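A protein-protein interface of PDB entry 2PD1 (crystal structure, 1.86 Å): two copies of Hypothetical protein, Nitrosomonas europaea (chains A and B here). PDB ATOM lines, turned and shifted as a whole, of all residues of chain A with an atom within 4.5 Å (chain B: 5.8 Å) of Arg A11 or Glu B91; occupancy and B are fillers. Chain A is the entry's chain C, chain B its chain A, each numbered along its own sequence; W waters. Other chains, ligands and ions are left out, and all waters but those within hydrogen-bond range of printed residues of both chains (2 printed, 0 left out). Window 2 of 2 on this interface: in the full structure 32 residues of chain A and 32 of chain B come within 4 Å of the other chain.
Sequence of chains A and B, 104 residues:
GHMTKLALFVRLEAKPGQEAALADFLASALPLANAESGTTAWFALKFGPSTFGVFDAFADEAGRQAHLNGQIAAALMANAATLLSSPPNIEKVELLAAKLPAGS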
ATOM      1  N   PHE A   9       1.364  34.405   1.693  1.00  0.00           N
ATOM      2  CA  PHE A   9       2.318  33.530   2.418  1.00  0.00           C
ATOM      3  C   PHE A   9       3.489  33.204   1.475  1.00  0.00           C
ATOM      4  O   PHE A   9       3.260  32.906   0.301  1.00  0.00           O
ATOM      5  CB  PHE A   9       1.643  32.235   2.841  1.00  0.00           C
ATOM      6  CG  PHE A   9       2.620  31.245   3.418  1.00  0.00           C
ATOM      7  CD1 PHE A   9       3.167  31.470   4.678  1.00  0.00           C
ATOM      8  CD2 PHE A   9       3.071  30.152   2.670  1.00  0.00           C
ATOM      9  CE1 PHE A   9       4.105  30.587   5.210  1.00  0.00           C
ATOM     10  CE2 PHE A   9       4.007  29.264   3.199  1.00  0.00           C
ATOM     11  CZ  PHE A   9       4.536  29.492   4.460  1.00  0.00           C
ATOM     12  N   VAL A  10       4.724  33.326   1.956  1.00  0.00           N
ATOM     13  CA  VAL A  10       5.854  32.971   1.143  1.00  0.00           C
ATOM     14  C   VAL A  10       6.850  32.205   2.016  1.00  0.00           C
ATOM     15  O   VAL A  10       7.145  32.619   3.179  1.00  0.00           O
ATOM     16  CB  VAL A  10       6.496  34.207   0.443  1.00  0.00           C
ATOM     17  CG1 VAL A  10       7.094  35.140   1.452  1.00  0.00           C
ATOM     18  CG2 VAL A  10       7.606  33.783  -0.592  1.00  0.00           C
ATOM     19  N   ARG A  11       7.369  31.095   1.496  1.00  0.00           N
ATOM     20  CA  ARG A  11       8.424  30.378   2.222  1.00  0.00           C
ATOM     21  C   ARG A  11       9.732  30.746   1.533  1.00  0.00           C
ATOM     22  O   ARG A  11       9.769  30.837   0.307  1.00  0.00           O
ATOM     23  CB  ARG A  11       8.196  28.864   2.211  1.00  0.00           C
ATOM     24  CG  ARG A  11       9.065  28.083   3.226  1.00  0.00           C
ATOM     25  CD  ARG A  11       8.752  26.573   3.120  1.00  0.00           C
ATOM     26  NE  ARG A  11       7.347  26.264   3.493  1.00  0.00           N
ATOM     27  CZ  ARG A  11       7.003  25.823   4.711  1.00  0.00           C
ATOM     28  NH1 ARG A  11       7.936  25.649   5.643  1.00  0.00           N
ATOM     29  NH2 ARG A  11       5.736  25.537   5.012  1.00  0.00           N
ATOM     30  N   LEU A  12      10.787  30.982   2.315  1.00  0.00           N
ATOM     31  CA  LEU A  12      12.097  31.510   1.787  1.00  0.00           C
ATOM     32  C   LEU A  12      13.246  30.635   2.255  1.00  0.00           C
ATOM     33  O   LEU A  12      13.371  30.398   3.465  1.00  0.00           O
ATOM     34  CB  LEU A  12      12.337  32.941   2.312  1.00  0.00           C
ATOM     35  CG  LEU A  12      11.263  34.002   2.003  1.00  0.00           C
ATOM     36  CD1 LEU A  12      11.365  35.216   2.902  1.00  0.00           C
ATOM     37  CD2 LEU A  12      11.398  34.483   0.586  1.00  0.00           C
ATOM     38  N   GLU A  13      14.085  30.144   1.322  1.00  0.00           N
ATOM     39  CA  GLU A  13      15.178  29.251   1.675  1.00  0.00           C
ATOM     40  C   GLU A  13      16.434  30.054   1.494  1.00  0.00           C
ATOM     41  O   GLU A  13      16.685  30.548   0.380  1.00  0.00           O
ATOM     42  CB  GLU A  13      15.184  28.038   0.737  1.00  0.00           C
ATOM     43  CG  GLU A  13      13.856  27.288   0.642  1.00  0.00           C
ATOM     44  CD  GLU A  13      13.460  26.579   1.926  1.00  0.00           C
ATOM     45  OE1 GLU A  13      14.311  26.446   2.866  1.00  0.00           O
ATOM     46  OE2 GLU A  13      12.279  26.134   1.974  1.00  0.00           O
ATOM     47  N   PHE A  47      11.222  28.912  10.282  1.00  0.00           N
ATOM     48  CA  PHE A  47      10.869  27.490  10.410  1.00  0.00           C
ATOM     49  C   PHE A  47      12.060  26.670  10.834  1.00  0.00           C
ATOM     50  O   PHE A  47      11.905  25.642  11.492  1.00  0.00           O
ATOM     51  CB  PHE A  47      10.364  26.917   9.076  1.00  0.00           C
ATOM     52  CG  PHE A  47       9.075  27.554   8.573  1.00  0.00           C
ATOM     53  CD1 PHE A  47       7.833  27.015   8.919  1.00  0.00           C
ATOM     54  CD2 PHE A  47       9.113  28.655   7.689  1.00  0.00           C
ATOM     55  CE1 PHE A  47       6.631  27.585   8.427  1.00  0.00           C
ATOM     56  CE2 PHE A  47       7.899  29.242   7.182  1.00  0.00           C
ATOM     57  CZ  PHE A  47       6.662  28.711   7.580  1.00  0.00           C
ATOM     58  N   THR A  51      15.395  28.164   6.663  1.00  0.00           N
ATOM     59  CA  THR A  51      14.059  28.213   6.054  1.00  0.00           C
ATOM     60  C   THR A  51      13.279  29.255   6.843  1.00  0.00           C
ATOM     61  O   THR A  51      13.138  29.159   8.082  1.00  0.00           O
ATOM     62  CB  THR A  51      13.309  26.862   6.086  1.00  0.00           C
ATOM     63  OG1 THR A  51      14.126  25.838   5.488  1.00  0.00           O
ATOM     64  CG2 THR A  51      12.029  26.958   5.258  1.00  0.00           C
ATOM     65  N   PHE A  52      12.779  30.248   6.108  1.00  0.00           N
ATOM     66  CA  PHE A  52      12.153  31.394   6.704  1.00  0.00           C
ATOM     67  C   PHE A  52      10.863  31.656   5.933  1.00  0.00           C
ATOM     68  O   PHE A  52      10.500  30.862   5.065  1.00  0.00           O
ATOM     69  CB  PHE A  52      13.112  32.610   6.683  1.00  0.00           C
ATOM     70  CG  PHE A  52      14.373  32.385   7.489  1.00  0.00           C
ATOM     71  CD1 PHE A  52      14.459  32.857   8.806  1.00  0.00           C
ATOM     72  CD2 PHE A  52      15.451  31.680   6.939  1.00  0.00           C
ATOM     73  CE1 PHE A  52      15.623  32.637   9.572  1.00  0.00           C
ATOM     74  CE2 PHE A  52      16.595  31.433   7.678  1.00  0.00           C
ATOM     75  CZ  PHE A  52      16.692  31.917   9.007  1.00  0.00           C
ATOM     76  N   GLY A  53      10.171  32.750   6.243  1.00  0.00           N
ATOM     77  CA  GLY A  53       8.940  33.077   5.523  1.00  0.00           C
ATOM     78  C   GLY A  53       8.279  34.359   6.018  1.00  0.00           C
ATOM     79  O   GLY A  53       8.792  35.017   6.941  1.00  0.00           O
ATOM     80  N   PRO A  88      11.239  31.773  -4.623  1.00  0.00           N
ATOM     81  CA  PRO A  88      10.063  31.547  -3.771  1.00  0.00           C
ATOM     82  C   PRO A  88       8.760  31.751  -4.537  1.00  0.00           C
ATOM     83  O   PRO A  88       8.682  32.626  -5.395  1.00  0.00           O
ATOM     84  CB  PRO A  88      10.220  32.616  -2.676  1.00  0.00           C
ATOM     85  CG  PRO A  88      10.919  33.766  -3.386  1.00  0.00           C
ATOM     86  CD  PRO A  88      11.847  33.098  -4.408  1.00  0.00           C
ATOM     87  N   ALA B   7       4.441  30.741  16.875  1.00  0.00           N
ATOM     88  CA  ALA B   7       3.340  30.554  15.930  1.00  0.00           C
ATOM     89  C   ALA B   7       3.197  29.095  15.532  1.00  0.00           C
ATOM     90  O   ALA B   7       4.074  28.242  15.863  1.00  0.00           O
ATOM     91  CB  ALA B   7       3.522  31.447  14.686  1.00  0.00           C
ATOM     92  N   LEU B   8       2.057  28.813  14.882  1.00  0.00           N
ATOM     93  CA  LEU B   8       1.821  27.514  14.221  1.00  0.00           C
ATOM     94  C   LEU B   8       1.390  27.816  12.842  1.00  0.00           C
ATOM     95  O   LEU B   8       0.647  28.780  12.629  1.00  0.00           O
ATOM     96  CB  LEU B   8       0.688  26.752  14.895  1.00  0.00           C
ATOM     97  CG  LEU B   8       0.997  26.367  16.328  1.00  0.00           C
ATOM     98  CD1 LEU B   8      -0.308  25.916  16.958  1.00  0.00           C
ATOM     99  CD2 LEU B   8       2.065  25.249  16.320  1.00  0.00           C
ATOM    100  N   PHE B   9       1.838  26.985  11.899  1.00  0.00           N
ATOM    101  CA  PHE B   9       1.408  27.103  10.552  1.00  0.00           C
ATOM    102  C   PHE B   9       0.877  25.719  10.211  1.00  0.00           C
ATOM    103  O   PHE B   9       1.632  24.763  10.206  1.00  0.00           O
ATOM    104  CB  PHE B   9       2.563  27.523   9.645  1.00  0.00           C
ATOM    105  CG  PHE B   9       2.172  27.601   8.188  1.00  0.00           C
ATOM    106  CD1 PHE B   9       1.288  28.579   7.740  1.00  0.00           C
ATOM    107  CD2 PHE B   9       2.725  26.725   7.257  1.00  0.00           C
ATOM    108  CE1 PHE B   9       0.924  28.665   6.363  1.00  0.00           C
ATOM    109  CE2 PHE B   9       2.376  26.791   5.902  1.00  0.00           C
ATOM    110  CZ  PHE B   9       1.478  27.771   5.445  1.00  0.00           C
ATOM    111  N   VAL B  10      -0.440  25.615  10.040  1.00  0.00           N
ATOM    112  CA  VAL B  10      -1.120  24.330   9.883  1.00  0.00           C
ATOM    113  C   VAL B  10      -1.695  24.233   8.478  1.00  0.00           C
ATOM    114  O   VAL B  10      -2.380  25.159   8.008  1.00  0.00           O
ATOM    115  CB  VAL B  10      -2.296  24.237  10.858  1.00  0.00           C
ATOM    116  CG1 VAL B  10      -2.946  22.854  10.795  1.00  0.00           C
ATOM    117  CG2 VAL B  10      -1.827  24.523  12.290  1.00  0.00           C
ATOM    118  N   ARG B  11      -1.404  23.145   7.779  1.00  0.00           N
ATOM    119  CA  ARG B  11      -2.093  22.914   6.484  1.00  0.00           C
ATOM    120  C   ARG B  11      -3.117  21.819   6.659  1.00  0.00           C
ATOM    121  O   ARG B  11      -2.863  20.838   7.369  1.00  0.00           O
ATOM    122  CB  ARG B  11      -1.125  22.588   5.343  1.00  0.00           C
ATOM    123  CG  ARG B  11      -0.353  23.801   4.893  1.00  0.00           C
ATOM    124  CD  ARG B  11      -0.070  23.762   3.404  1.00  0.00           C
ATOM    125  NE  ARG B  11       0.961  24.737   3.048  1.00  0.00           N
ATOM    126  CZ  ARG B  11       0.883  25.619   2.046  1.00  0.00           C
ATOM    127  NH1 ARG B  11      -0.194  25.669   1.266  1.00  0.00           N
ATOM    128  NH2 ARG B  11       1.895  26.447   1.820  1.00  0.00           N
ATOM    129  N   ASN B  89      -1.208  18.997   8.950  1.00  0.00           N
ATOM    130  CA  ASN B  89       0.244  19.144   8.908  1.00  0.00           C
ATOM    131  C   ASN B  89       0.649  20.398   9.702  1.00  0.00           C
ATOM    132  O   ASN B  89       0.439  21.514   9.229  1.00  0.00           O
ATOM    133  CB  ASN B  89       0.761  19.269   7.480  1.00  0.00           C
ATOM    134  CG  ASN B  89       2.288  19.246   7.444  1.00  0.00           C
ATOM    135  OD1 ASN B  89       2.948  20.282   7.574  1.00  0.00           O
ATOM    136  ND2 ASN B  89       2.844  18.047   7.429  1.00  0.00           N
ATOM    137  N   ILE B  90       1.204  20.206  10.903  1.00  0.00           N
ATOM    138  CA  ILE B  90       1.426  21.302  11.849  1.00  0.00           C
ATOM    139  C   ILE B  90       2.909  21.605  11.968  1.00  0.00           C
ATOM    140  O   ILE B  90       3.706  20.701  12.263  1.00  0.00           O
ATOM    141  CB  ILE B  90       0.849  20.987  13.214  1.00  0.00           C
ATOM    142  CG1 ILE B  90      -0.622  20.633  13.064  1.00  0.00           C
ATOM    143  CG2 ILE B  90       1.060  22.189  14.177  1.00  0.00           C
ATOM    144  CD1 ILE B  90      -1.202  20.063  14.323  1.00  0.00           C
ATOM    145  N   GLU B  91       3.273  22.840  11.618  1.00  0.00           N
ATOM    146  CA  GLU B  91       4.638  23.347  11.765  1.00  0.00           C
ATOM    147  C   GLU B  91       4.755  24.370  12.877  1.00  0.00           C
ATOM    148  O   GLU B  91       4.065  25.400  12.887  1.00  0.00           O
ATOM    149  CB  GLU B  91       5.153  23.988  10.458  1.00  0.00           C
ATOM    150  CG  GLU B  91       5.428  22.985   9.358  1.00  0.00           C
ATOM    151  CD  GLU B  91       5.820  23.682   8.043  1.00  0.00           C
ATOM    152  OE1 GLU B  91       7.043  23.911   7.848  1.00  0.00           O
ATOM    153  OE2 GLU B  91       4.901  24.004   7.219  1.00  0.00           O
ATOM    154  N   LYS B  92       5.656  24.104  13.804  1.00  0.00           N
ATOM    155  CA  LYS B  92       6.004  25.084  14.834  1.00  0.00           C
ATOM    156  C   LYS B  92       6.905  26.138  14.216  1.00  0.00           C
ATOM    157  O   LYS B  92       7.889  25.822  13.510  1.00  0.00           O
ATOM    158  CB  LYS B  92       6.677  24.408  16.001  1.00  0.00           C
ATOM    159  CG  LYS B  92       5.701  23.528  16.786  1.00  0.00           C
ATOM    160  CD  LYS B  92       6.412  22.881  17.964  1.00  0.00           C
ATOM    161  CE  LYS B  92       5.421  22.504  19.076  1.00  0.00           C
ATOM    162  NZ  LYS B  92       4.343  21.546  18.650  1.00  0.00           N
ATOM    163  N   VAL B  93       6.564  27.393  14.479  1.00  0.00           N
ATOM    164  CA  VAL B  93       7.220  28.532  13.853  1.00  0.00           C
ATOM    165  C   VAL B  93       7.709  29.516  14.923  1.00  0.00           C
ATOM    166  O   VAL B  93       7.040  29.732  15.933  1.00  0.00           O
ATOM    167  CB  VAL B  93       6.235  29.237  12.861  1.00  0.00           C
ATOM    168  CG1 VAL B  93       6.858  30.513  12.261  1.00  0.00           C
ATOM    169  CG2 VAL B  93       5.836  28.269  11.763  1.00  0.00           C
HETATM  170  O   HOH W   1       3.894  25.102   2.773  1.00  0.00           O
HETATM  171  O   HOH W   2       9.276  24.557  11.778  1.00  0.00           O
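Phe A9 touches its own counterpart, Phe B9. Phe A9 touches Arg B11, and with the chains exchanged Arg A11 touches Phe B9. Of the 6 pairs that touch across the chains among the printed residues, 3 have their exchanged pair printed and touching as well.
Phe B9 touches Phe A9 (CZ to CZ, 3.6 Å). CE2 of Phe A9 touches NH2 of Arg B11 (3.8 Å). Arg A11 touches Phe B9. Glu B91 touches Phe A47. CE1 of Phe A47 touches CG2 of Val B93, 3.5 Å away.
The backbone NH (N) of Arg B11 sits at hydrogen-bond distance from the backbone carbonyl oxygen (O) of Asn B89, at 2.9 Å. O of Phe B9 lies within hydrogen-bond range of N of Glu B91 (2.9 Å). The backbone NH (N) of Ala B7 sits at hydrogen-bond distance from the backbone carbonyl oxygen (O) of Val B93 (2.9 Å).
Hydrophobic or aromatic side chains of chain A within 4 Å of the printed part of chain B: Phe A9 and Phe A47.
The guanidinium group (NH2) of Arg A11 lies within salt-bridge range of the side-chain carboxylate (OE2) of Glu B91 (2.8 Å).
Water W2 bridges O of Lys B92 (2.6 Å) and O of Phe A47 (2.9 Å). Water W1 lies within hydrogen-bond range of NH2 of Arg B11 and NH2 of Arg A11.
Arg A11 touches two residues of chain B. Glu B91 touches two residues of chain A. Printed residues of chain B within 4 Å of Phe A47: Glu B91 and Val B93. Printed residues of chain A within 4 Å of Val B93: Phe A47 (3.5 Å). Of the printed residues of chain A, Arg B11 touches Phe A9. Ala B7 touches none of the printed residues of chain A. The nearest printed residue of chain A that does not touch Glu B91 is Phe A9 (6.2 Å). The nearest printed residue of chain A that does not touch Val B93 is Arg A11 (7.0 Å).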
